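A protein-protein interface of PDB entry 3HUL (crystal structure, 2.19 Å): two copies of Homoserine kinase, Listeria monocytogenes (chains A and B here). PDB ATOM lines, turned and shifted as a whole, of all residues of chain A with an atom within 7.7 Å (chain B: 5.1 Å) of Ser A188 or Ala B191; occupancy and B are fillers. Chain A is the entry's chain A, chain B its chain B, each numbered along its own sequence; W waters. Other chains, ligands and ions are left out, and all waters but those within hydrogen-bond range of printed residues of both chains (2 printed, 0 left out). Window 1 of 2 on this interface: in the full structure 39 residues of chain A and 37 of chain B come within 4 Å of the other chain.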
ATOM      1  N   PRO A  16      10.496   3.169  -6.329  1.00  0.00           N
ATOM      2  CA  PRO A  16       9.177   2.721  -6.668  1.00  0.00           C
ATOM      3  C   PRO A  16       8.354   3.834  -7.308  1.00  0.00           C
ATOM      4  O   PRO A  16       7.142   3.679  -7.441  1.00  0.00           O
ATOM      5  CB  PRO A  16       8.596   2.294  -5.313  1.00  0.00           C
ATOM      6  CG  PRO A  16       9.700   2.500  -4.310  1.00  0.00           C
ATOM      7  CD  PRO A  16      10.554   3.555  -4.916  1.00  0.00           C
ATOM      8  N   GLY A  17       8.997   4.915  -7.760  1.00  0.00           N
ATOM      9  CA  GLY A  17       8.302   5.945  -8.557  1.00  0.00           C
ATOM     10  C   GLY A  17       8.000   5.516  -9.993  1.00  0.00           C
ATOM     11  O   GLY A  17       8.264   6.250 -10.955  1.00  0.00           O
ATOM     12  N   SER A  20       6.514   7.558 -12.861  1.00  0.00           N
ATOM     13  CA  SER A  20       6.255   8.768 -12.113  1.00  0.00           C
ATOM     14  C   SER A  20       7.467   9.682 -11.938  1.00  0.00           C
ATOM     15  O   SER A  20       7.409  10.867 -12.297  1.00  0.00           O
ATOM     16  CB  SER A  20       5.631   8.428 -10.764  1.00  0.00           C
ATOM     17  OG  SER A  20       5.415   9.620 -10.030  1.00  0.00           O
ATOM     18  N   VAL A 137       8.411  14.790 -10.620  1.00  0.00           N
ATOM     19  CA  VAL A 137       7.452  13.816 -10.109  1.00  0.00           C
ATOM     20  C   VAL A 137       6.173  13.999 -10.921  1.00  0.00           C
ATOM     21  O   VAL A 137       5.607  15.101 -10.977  1.00  0.00           O
ATOM     22  CB  VAL A 137       7.158  14.018  -8.601  1.00  0.00           C
ATOM     23  CG1 VAL A 137       6.037  13.066  -8.101  1.00  0.00           C
ATOM     24  CG2 VAL A 137       8.410  13.875  -7.782  1.00  0.00           C
ATOM     25  N   GLY A 138       5.709  12.918 -11.535  1.00  0.00           N
ATOM     26  CA  GLY A 138       4.647  13.001 -12.523  1.00  0.00           C
ATOM     27  C   GLY A 138       3.567  11.973 -12.350  1.00  0.00           C
ATOM     28  O   GLY A 138       3.742  10.948 -11.674  1.00  0.00           O
ATOM     29  N   ALA A 139       2.428  12.257 -12.964  1.00  0.00           N
ATOM     30  CA  ALA A 139       1.334  11.289 -13.076  1.00  0.00           C
ATOM     31  C   ALA A 139       0.607  11.481 -14.416  1.00  0.00           C
ATOM     32  O   ALA A 139       0.272  12.600 -14.828  1.00  0.00           O
ATOM     33  CB  ALA A 139       0.373  11.401 -11.906  1.00  0.00           C
ATOM     34  N   LEU A 141      -2.692  10.301 -16.165  1.00  0.00           N
ATOM     35  CA  LEU A 141      -3.975   9.797 -15.665  1.00  0.00           C
ATOM     36  C   LEU A 141      -4.955   9.953 -16.791  1.00  0.00           C
ATOM     37  O   LEU A 141      -5.400  11.084 -17.098  1.00  0.00           O
ATOM     38  CB  LEU A 141      -4.482  10.624 -14.481  1.00  0.00           C
ATOM     39  CG  LEU A 141      -3.508  10.924 -13.342  1.00  0.00           C
ATOM     40  CD1 LEU A 141      -4.168  11.852 -12.308  1.00  0.00           C
ATOM     41  CD2 LEU A 141      -3.022   9.641 -12.702  1.00  0.00           C
ATOM     42  N   LYS A 182      -2.721  -4.623  -0.855  1.00  0.00           N
ATOM     43  CA  LYS A 182      -1.813  -4.242   0.216  1.00  0.00           C
ATOM     44  C   LYS A 182      -0.408  -3.957  -0.317  1.00  0.00           C
ATOM     45  O   LYS A 182       0.288  -3.069   0.178  1.00  0.00           O
ATOM     46  CB  LYS A 182      -1.771  -5.336   1.290  1.00  0.00           C
ATOM     47  CG  LYS A 182      -0.879  -5.012   2.475  1.00  0.00           C
ATOM     48  CD  LYS A 182      -1.061  -5.995   3.631  1.00  0.00           C
ATOM     49  CE  LYS A 182      -0.828  -5.296   4.980  1.00  0.00           C
ATOM     50  NZ  LYS A 182       0.477  -4.557   5.035  1.00  0.00           N
ATOM     51  N   GLU A 183       0.000  -4.728  -1.320  1.00  0.00           N
ATOM     52  CA  GLU A 183       1.321  -4.590  -1.917  1.00  0.00           C
ATOM     53  C   GLU A 183       1.423  -3.255  -2.639  1.00  0.00           C
ATOM     54  O   GLU A 183       2.436  -2.575  -2.534  1.00  0.00           O
ATOM     55  CB  GLU A 183       1.562  -5.731  -2.900  1.00  0.00           C
ATOM     56  CG  GLU A 183       3.032  -5.978  -3.262  1.00  0.00           C
ATOM     57  CD  GLU A 183       3.257  -7.391  -3.830  1.00  0.00           C
ATOM     58  OE1 GLU A 183       2.924  -8.378  -3.129  1.00  0.00           O
ATOM     59  OE2 GLU A 183       3.756  -7.509  -4.971  1.00  0.00           O
ATOM     60  N   ALA A 184       0.371  -2.897  -3.368  1.00  0.00           N
ATOM     61  CA  ALA A 184       0.324  -1.637  -4.086  1.00  0.00           C
ATOM     62  C   ALA A 184       0.383  -0.429  -3.135  1.00  0.00           C
ATOM     63  O   ALA A 184       1.106   0.531  -3.400  1.00  0.00           O
ATOM     64  CB  ALA A 184      -0.922  -1.570  -4.963  1.00  0.00           C
ATOM     65  N   VAL A 185      -0.385  -0.497  -2.038  1.00  0.00           N
ATOM     66  CA  VAL A 185      -0.437   0.556  -1.014  1.00  0.00           C
ATOM     67  C   VAL A 185       0.952   0.777  -0.422  1.00  0.00           C
ATOM     68  O   VAL A 185       1.404   1.908  -0.298  1.00  0.00           O
ATOM     69  CB  VAL A 185      -1.470   0.234   0.098  1.00  0.00           C
ATOM     70  CG1 VAL A 185      -1.386   1.231   1.254  1.00  0.00           C
ATOM     71  CG2 VAL A 185      -2.892   0.246  -0.480  1.00  0.00           C
ATOM     72  N   GLN A 186       1.628  -0.322  -0.118  1.00  0.00           N
ATOM     73  CA  GLN A 186       2.962  -0.304   0.432  1.00  0.00           C
ATOM     74  C   GLN A 186       4.007   0.268  -0.549  1.00  0.00           C
ATOM     75  O   GLN A 186       4.870   1.066  -0.151  1.00  0.00           O
ATOM     76  CB  GLN A 186       3.339  -1.710   0.893  1.00  0.00           C
ATOM     77  CG  GLN A 186       4.800  -1.881   1.240  1.00  0.00           C
ATOM     78  CD  GLN A 186       5.093  -3.169   2.025  1.00  0.00           C
ATOM     79  OE1 GLN A 186       4.597  -3.361   3.145  1.00  0.00           O
ATOM     80  NE2 GLN A 186       5.949  -4.029   1.457  1.00  0.00           N
ATOM     81  N   ALA A 187       3.928  -0.123  -1.818  1.00  0.00           N
ATOM     82  CA  ALA A 187       4.873   0.383  -2.814  1.00  0.00           C
ATOM     83  C   ALA A 187       4.687   1.886  -2.999  1.00  0.00           C
ATOM     84  O   ALA A 187       5.642   2.619  -3.222  1.00  0.00           O
ATOM     85  CB  ALA A 187       4.696  -0.319  -4.134  1.00  0.00           C
ATOM     86  N   SER A 188       3.444   2.326  -2.930  1.00  0.00           N
ATOM     87  CA  SER A 188       3.163   3.738  -3.013  1.00  0.00           C
ATOM     88  C   SER A 188       3.828   4.463  -1.847  1.00  0.00           C
ATOM     89  O   SER A 188       4.500   5.470  -2.033  1.00  0.00           O
ATOM     90  CB  SER A 188       1.654   3.980  -3.024  1.00  0.00           C
ATOM     91  OG  SER A 188       1.400   5.359  -3.157  1.00  0.00           O
ATOM     92  N   SER A 189       3.689   3.900  -0.647  1.00  0.00           N
ATOM     93  CA  SER A 189       4.171   4.562   0.566  1.00  0.00           C
ATOM     94  C   SER A 189       5.681   4.703   0.541  1.00  0.00           C
ATOM     95  O   SER A 189       6.215   5.680   1.035  1.00  0.00           O
ATOM     96  CB  SER A 189       3.683   3.836   1.826  1.00  0.00           C
ATOM     97  OG  SER A 189       4.303   2.567   1.933  1.00  0.00           O
ATOM     98  N   ILE A 190       6.364   3.767  -0.105  1.00  0.00           N
ATOM     99  CA  ILE A 190       7.830   3.840  -0.239  1.00  0.00           C
ATOM    100  C   ILE A 190       8.303   4.961  -1.181  1.00  0.00           C
ATOM    101  O   ILE A 190       9.313   5.634  -0.921  1.00  0.00           O
ATOM    102  CB  ILE A 190       8.397   2.456  -0.686  1.00  0.00           C
ATOM    103  CG1 ILE A 190       8.072   1.380   0.368  1.00  0.00           C
ATOM    104  CG2 ILE A 190       9.915   2.528  -1.001  1.00  0.00           C
ATOM    105  CD1 ILE A 190       8.545   1.699   1.803  1.00  0.00           C
ATOM    106  N   ALA A 191       7.595   5.141  -2.301  1.00  0.00           N
ATOM    107  CA  ALA A 191       7.900   6.248  -3.193  1.00  0.00           C
ATOM    108  C   ALA A 191       7.577   7.587  -2.482  1.00  0.00           C
ATOM    109  O   ALA A 191       8.344   8.535  -2.568  1.00  0.00           O
ATOM    110  CB  ALA A 191       7.118   6.101  -4.488  1.00  0.00           C
ATOM    111  N   ASN A 192       6.448   7.643  -1.785  1.00  0.00           N
ATOM    112  CA  ASN A 192       6.063   8.829  -0.989  1.00  0.00           C
ATOM    113  C   ASN A 192       7.187   9.226  -0.032  1.00  0.00           C
ATOM    114  O   ASN A 192       7.589  10.380   0.012  1.00  0.00           O
ATOM    115  CB  ASN A 192       4.821   8.564  -0.151  1.00  0.00           C
ATOM    116  CG  ASN A 192       3.591   8.301  -0.966  1.00  0.00           C
ATOM    117  OD1 ASN A 192       3.570   8.489  -2.186  1.00  0.00           O
ATOM    118  ND2 ASN A 192       2.515   7.901  -0.279  1.00  0.00           N
ATOM    119  N   VAL A 193       7.691   8.255   0.724  1.00  0.00           N
ATOM    120  CA  VAL A 193       8.779   8.495   1.665  1.00  0.00           C
ATOM    121  C   VAL A 193      10.064   8.952   0.950  1.00  0.00           C
ATOM    122  O   VAL A 193      10.720   9.906   1.382  1.00  0.00           O
ATOM    123  CB  VAL A 193       9.028   7.255   2.580  1.00  0.00           C
ATOM    124  CG1 VAL A 193      10.297   7.456   3.431  1.00  0.00           C
ATOM    125  CG2 VAL A 193       7.834   7.049   3.497  1.00  0.00           C
ATOM    126  N   MET A 194      10.388   8.305  -0.169  1.00  0.00           N
ATOM    127  CA  MET A 194      11.556   8.664  -0.982  1.00  0.00           C
ATOM    128  C   MET A 194      11.451  10.131  -1.364  1.00  0.00           C
ATOM    129  O   MET A 194      12.398  10.892  -1.155  1.00  0.00           O
ATOM    130  CB  MET A 194      11.636   7.810  -2.244  1.00  0.00           C
ATOM    131  CG  MET A 194      12.803   8.156  -3.199  1.00  0.00           C
ATOM    132  SD  MET A 194      12.831   7.227  -4.774  1.00  0.00           S
ATOM    133  CE  MET A 194      11.551   8.048  -5.715  1.00  0.00           C
ATOM    134  N   ILE A 195      10.303  10.536  -1.915  1.00  0.00           N
ATOM    135  CA  ILE A 195      10.098  11.934  -2.304  1.00  0.00           C
ATOM    136  C   ILE A 195      10.216  12.881  -1.086  1.00  0.00           C
ATOM    137  O   ILE A 195      10.937  13.867  -1.117  1.00  0.00           O
ATOM    138  CB  ILE A 195       8.718  12.136  -3.009  1.00  0.00           C
ATOM    139  CG1 ILE A 195       8.677  11.422  -4.366  1.00  0.00           C
ATOM    140  CG2 ILE A 195       8.402  13.591  -3.163  1.00  0.00           C
ATOM    141  CD1 ILE A 195       7.241  11.052  -4.824  1.00  0.00           C
ATOM    142  N   LEU A 214       9.409  -3.476  -5.813  1.00  0.00           N
ATOM    143  CA  LEU A 214       8.003  -3.607  -5.382  1.00  0.00           C
ATOM    144  C   LEU A 214       6.909  -3.676  -6.444  1.00  0.00           C
ATOM    145  O   LEU A 214       5.792  -4.120  -6.140  1.00  0.00           O
ATOM    146  CB  LEU A 214       7.647  -2.584  -4.295  1.00  0.00           C
ATOM    147  CG  LEU A 214       8.475  -2.579  -3.007  1.00  0.00           C
ATOM    148  CD1 LEU A 214       8.189  -1.294  -2.245  1.00  0.00           C
ATOM    149  CD2 LEU A 214       8.203  -3.811  -2.133  1.00  0.00           C
ATOM    150  N   TRP A 215       7.212  -3.266  -7.670  1.00  0.00           N
ATOM    151  CA  TRP A 215       6.167  -3.057  -8.682  1.00  0.00           C
ATOM    152  C   TRP A 215       5.882  -4.198  -9.689  1.00  0.00           C
ATOM    153  O   TRP A 215       6.646  -5.156  -9.810  1.00  0.00           O
ATOM    154  CB  TRP A 215       6.400  -1.735  -9.420  1.00  0.00           C
ATOM    155  CG  TRP A 215       6.000  -0.535  -8.618  1.00  0.00           C
ATOM    156  CD1 TRP A 215       6.826   0.420  -8.108  1.00  0.00           C
ATOM    157  CD2 TRP A 215       4.673  -0.165  -8.222  1.00  0.00           C
ATOM    158  NE1 TRP A 215       6.104   1.368  -7.439  1.00  0.00           N
ATOM    159  CE2 TRP A 215       4.778   1.035  -7.487  1.00  0.00           C
ATOM    160  CE3 TRP A 215       3.402  -0.734  -8.413  1.00  0.00           C
ATOM    161  CZ2 TRP A 215       3.674   1.679  -6.945  1.00  0.00           C
ATOM    162  CZ3 TRP A 215       2.297  -0.087  -7.871  1.00  0.00           C
ATOM    163  CH2 TRP A 215       2.443   1.106  -7.144  1.00  0.00           C
ATOM    164  N   PRO B  16      -5.189  10.096  -1.820  1.00  0.00           N
ATOM    165  CA  PRO B  16      -4.281   9.098  -2.403  1.00  0.00           C
ATOM    166  C   PRO B  16      -3.100   8.703  -1.503  1.00  0.00           C
ATOM    167  O   PRO B  16      -2.486   7.653  -1.738  1.00  0.00           O
ATOM    168  CB  PRO B  16      -3.787   9.788  -3.671  1.00  0.00           C
ATOM    169  CG  PRO B  16      -3.910  11.252  -3.345  1.00  0.00           C
ATOM    170  CD  PRO B  16      -5.199  11.340  -2.610  1.00  0.00           C
ATOM    171  N   GLY B  17      -2.801   9.503  -0.479  1.00  0.00           N
ATOM    172  CA  GLY B  17      -1.816   9.123   0.548  1.00  0.00           C
ATOM    173  C   GLY B  17      -2.312   8.081   1.553  1.00  0.00           C
ATOM    174  O   GLY B  17      -1.767   7.953   2.655  1.00  0.00           O
ATOM    175  N   ALA B 187      -2.497   5.269  -8.971  1.00  0.00           N
ATOM    176  CA  ALA B 187      -2.847   5.653  -7.609  1.00  0.00           C
ATOM    177  C   ALA B 187      -1.604   6.130  -6.859  1.00  0.00           C
ATOM    178  O   ALA B 187      -1.647   7.133  -6.186  1.00  0.00           O
ATOM    179  CB  ALA B 187      -3.491   4.468  -6.866  1.00  0.00           C
ATOM    180  N   SER B 188      -0.508   5.387  -6.979  1.00  0.00           N
ATOM    181  CA  SER B 188       0.762   5.763  -6.355  1.00  0.00           C
ATOM    182  C   SER B 188       1.277   7.101  -6.912  1.00  0.00           C
ATOM    183  O   SER B 188       1.684   7.985  -6.163  1.00  0.00           O
ATOM    184  CB  SER B 188       1.792   4.672  -6.590  1.00  0.00           C
ATOM    185  OG  SER B 188       2.974   4.941  -5.860  1.00  0.00           O
ATOM    186  N   SER B 189       1.212   7.273  -8.226  1.00  0.00           N
ATOM    187  CA  SER B 189       1.758   8.485  -8.828  1.00  0.00           C
ATOM    188  C   SER B 189       0.945   9.740  -8.520  1.00  0.00           C
ATOM    189  O   SER B 189       1.485  10.824  -8.496  1.00  0.00           O
ATOM    190  CB  SER B 189       1.987   8.314 -10.326  1.00  0.00           C
ATOM    191  OG  SER B 189       0.762   8.241 -10.979  1.00  0.00           O
ATOM    192  N   ILE B 190      -0.341   9.594  -8.277  1.00  0.00           N
ATOM    193  CA  ILE B 190      -1.179  10.701  -7.787  1.00  0.00           C
ATOM    194  C   ILE B 190      -0.776  11.127  -6.382  1.00  0.00           C
ATOM    195  O   ILE B 190      -0.698  12.320  -6.096  1.00  0.00           O
ATOM    196  CB  ILE B 190      -2.691  10.266  -7.740  1.00  0.00           C
ATOM    197  CG1 ILE B 190      -3.238  10.115  -9.159  1.00  0.00           C
ATOM    198  CG2 ILE B 190      -3.549  11.291  -6.982  1.00  0.00           C
ATOM    199  CD1 ILE B 190      -4.620   9.401  -9.232  1.00  0.00           C
ATOM    200  N   ALA B 191      -0.573  10.151  -5.494  1.00  0.00           N
ATOM    201  CA  ALA B 191      -0.038  10.413  -4.150  1.00  0.00           C
ATOM    202  C   ALA B 191       1.326  11.108  -4.263  1.00  0.00           C
ATOM    203  O   ALA B 191       1.593  12.078  -3.537  1.00  0.00           O
ATOM    204  CB  ALA B 191       0.128   9.077  -3.350  1.00  0.00           C
ATOM    205  N   ASN B 192       2.165  10.587  -5.171  1.00  0.00           N
ATOM    206  CA  ASN B 192       3.511  11.133  -5.419  1.00  0.00           C
ATOM    207  C   ASN B 192       3.436  12.610  -5.766  1.00  0.00           C
ATOM    208  O   ASN B 192       4.155  13.428  -5.194  1.00  0.00           O
ATOM    209  CB  ASN B 192       4.188  10.407  -6.587  1.00  0.00           C
ATOM    210  CG  ASN B 192       4.635   8.976  -6.257  1.00  0.00           C
ATOM    211  OD1 ASN B 192       5.108   8.256  -7.139  1.00  0.00           O
ATOM    212  ND2 ASN B 192       4.507   8.578  -5.031  1.00  0.00           N
ATOM    213  N   VAL B 193       2.588  12.941  -6.745  1.00  0.00           N
ATOM    214  CA  VAL B 193       2.439  14.315  -7.208  1.00  0.00           C
ATOM    215  C   VAL B 193       1.831  15.195  -6.089  1.00  0.00           C
ATOM    216  O   VAL B 193       2.294  16.318  -5.879  1.00  0.00           O
ATOM    217  CB  VAL B 193       1.575  14.380  -8.507  1.00  0.00           C
ATOM    218  CG1 VAL B 193       1.201  15.838  -8.878  1.00  0.00           C
ATOM    219  CG2 VAL B 193       2.309  13.708  -9.661  1.00  0.00           C
ATOM    220  N   MET B 194       0.818  14.678  -5.374  1.00  0.00           N
ATOM    221  CA  MET B 194       0.231  15.390  -4.222  1.00  0.00           C
ATOM    222  C   MET B 194       1.360  15.793  -3.258  1.00  0.00           C
ATOM    223  O   MET B 194       1.496  16.946  -2.883  1.00  0.00           O
ATOM    224  CB  MET B 194      -0.757  14.502  -3.476  1.00  0.00           C
ATOM    225  CG  MET B 194      -1.402  15.221  -2.271  1.00  0.00           C
ATOM    226  SD  MET B 194      -2.604  14.250  -1.344  1.00  0.00           S
ATOM    227  CE  MET B 194      -1.575  13.082  -0.520  1.00  0.00           C
ATOM    228  N   ILE B 195       2.212  14.836  -2.916  1.00  0.00           N
ATOM    229  CA  ILE B 195       3.258  15.112  -1.959  1.00  0.00           C
ATOM    230  C   ILE B 195       4.239  16.133  -2.511  1.00  0.00           C
ATOM    231  O   ILE B 195       4.589  17.068  -1.823  1.00  0.00           O
ATOM    232  CB  ILE B 195       3.916  13.817  -1.522  1.00  0.00           C
ATOM    233  CG1 ILE B 195       2.896  13.023  -0.688  1.00  0.00           C
ATOM    234  CG2 ILE B 195       5.186  14.077  -0.734  1.00  0.00           C
ATOM    235  CD1 ILE B 195       3.234  11.560  -0.539  1.00  0.00           C
ATOM    236  N   ALA B 196       4.647  15.982  -3.770  1.00  0.00           N
ATOM    237  CA  ALA B 196       5.606  16.913  -4.351  1.00  0.00           C
ATOM    238  C   ALA B 196       5.018  18.314  -4.380  1.00  0.00           C
ATOM    239  O   ALA B 196       5.761  19.324  -4.244  1.00  0.00           O
ATOM    240  CB  ALA B 196       6.012  16.469  -5.754  1.00  0.00           C
ATOM    241  N   TRP B 215      -7.609   4.646  -4.591  1.00  0.00           N
ATOM    242  CA  TRP B 215      -7.542   3.419  -3.789  1.00  0.00           C
ATOM    243  C   TRP B 215      -8.928   2.834  -3.474  1.00  0.00           C
ATOM    244  O   TRP B 215      -9.939   3.252  -4.052  1.00  0.00           O
ATOM    245  CB  TRP B 215      -6.748   3.649  -2.487  1.00  0.00           C
ATOM    246  CG  TRP B 215      -5.345   4.146  -2.726  1.00  0.00           C
ATOM    247  CD1 TRP B 215      -4.872   5.406  -2.491  1.00  0.00           C
ATOM    248  CD2 TRP B 215      -4.244   3.401  -3.276  1.00  0.00           C
ATOM    249  NE1 TRP B 215      -3.545   5.489  -2.849  1.00  0.00           N
ATOM    250  CE2 TRP B 215      -3.134   4.276  -3.332  1.00  0.00           C
ATOM    251  CE3 TRP B 215      -4.087   2.081  -3.727  1.00  0.00           C
ATOM    252  CZ2 TRP B 215      -1.880   3.871  -3.818  1.00  0.00           C
ATOM    253  CZ3 TRP B 215      -2.838   1.683  -4.212  1.00  0.00           C
ATOM    254  CH2 TRP B 215      -1.753   2.578  -4.249  1.00  0.00           C
HETATM  255  O   HOH W   1       5.043   5.389  -7.535  1.00  0.00           O
HETATM  256  O   HOH W   2       0.014   6.424  -1.170  1.00  0.00           O
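OG of Ser A188 lies close to OG of Ser B188 (3.2 Å).
The side-chain amide oxygen of Asn B192 lies within hydrogen-bond range of the side-chain hydroxyl of Ser A20 (3.2 Å).
The side-chain amide oxygen of Asn A192 sits at hydrogen-bond distance from the side-chain amide nitrogen of Asn B192 (3.0 Å).
Water W2 lies within hydrogen-bond range of the side-chain hydroxyl of Ser A188 (2.6 Å), the backbone carbonyl oxygen of Pro B16 (2.8 Å) and the side-chain amide nitrogen of Asn A192 (3.0 Å).
Water W1 lies within hydrogen-bond range of the side-chain hydroxyl (OG) of Ser B188 (2.7 Å), the backbone carbonyl oxygen (O) of Pro A16 (2.7 Å) and the side-chain amide oxygen (OD1) of Asn B192 (2.9 Å).
Of the 13 printed residues of chain B, 9 touch a printed residue of chain A.
Hydrophobic or aromatic side chains of chain B that line the printed part of chain A: Ile B190, Ala B191, Val B193, Ile B195, Ala B196 and Trp B215.
Among the printed residues, no Asp or Glu carboxylate lies within 4 Å of a Lys or Arg side-chain nitrogen of the other chain.
Printed residues of chain B within 4 Å of Ser A20: Ser B189 and Asn B192.
Of the printed residues of chain B, Trp A215 touches Ser B188 (3.5 Å).
Of the printed residues of chain B, Ala A139 touches Ser B189 (3.3 Å) and Val B193 (3.6 Å).
Printed residues of chain B within 4 Å of Asn A192: Ala B191 (3.7 Å), Asn B192 (3.0 Å) and Ile B195 (3.3 Å).
Val A193 touches none of the printed residues of chain B.
The nearest residue of chain B that does not touch Ser A188 is Asn B192 (4.3 Å).
The nearest printed residue of chain A that does not touch Val B193 is Ser A20 (5.1 Å).
Ser A188 touches its own counterpart, Ser B188.
Ser A188 touches Ala B191, but with the chains exchanged Ala A191 does not touch Ser B188 (4.5 Å).
Ser A188 touches Trp B215, and with the chains exchanged Trp A215 touches Ser B188.
Asn B192 touches its own counterpart, Asn A192.
Of the 21 pairs that touch across the chains among the printed residues, 8 have their exchanged pair printed and touching as well.
Among the printed residues, merely in contact across the chains: Asn A192 with Ile B195 (3.3 Å), Ala A139 with Ser B189 (3.3 Å), Gly A138 with Val B193 (3.4 Å), Gly A138 with Ser B189 (3.4 Å), Val A137 with Asn B192 (3.5 Å), Trp A215 with Ser B188 (3.5 Å), Leu A141 with Ile B190 (3.6 Å), Ile A195 with Asn B192 (3.6 Å), Ala A139 with Val B193 (3.6 Å), Ala A184 with Trp B215 (3.6 Å), Ser A188 with Trp B215 (3.6 Å), Ala A191 with Asn B192 (3.6 Å), Ser A20 with Ser B189 (3.7 Å), Asn A192 with Ala B191 (3.7 Å), Val A137 with Val B193 (3.7 Å), Val A185 with Trp B215 (3.9 Å), Val A137 with Ala B196 (3.9 Å) and Ser A188 with Ala B191 (3.9 Å).
OG of Ser A20 lies within hydrogen-bond range of O of Gly A138 (2.7 Å).
The indole nitrogen (NE1) of Trp A215 sits at hydrogen-bond distance from the backbone carbonyl oxygen (O) of Pro A16 (2.5 Å).
The backbone carbonyl oxygen of Ser B188 lies within hydrogen-bond range of the side-chain amide nitrogen of Asn B192, at 3.1 Å.
The backbone carbonyl oxygen (O) of Ser A188 sits close to the side-chain amide oxygen (OD1) of Asn A192 (3.2 Å).
The backbone carbonyl oxygen of Pro B16 is in hydrogen-bond range of the indole nitrogen of Trp B215, 2.7 Å away.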
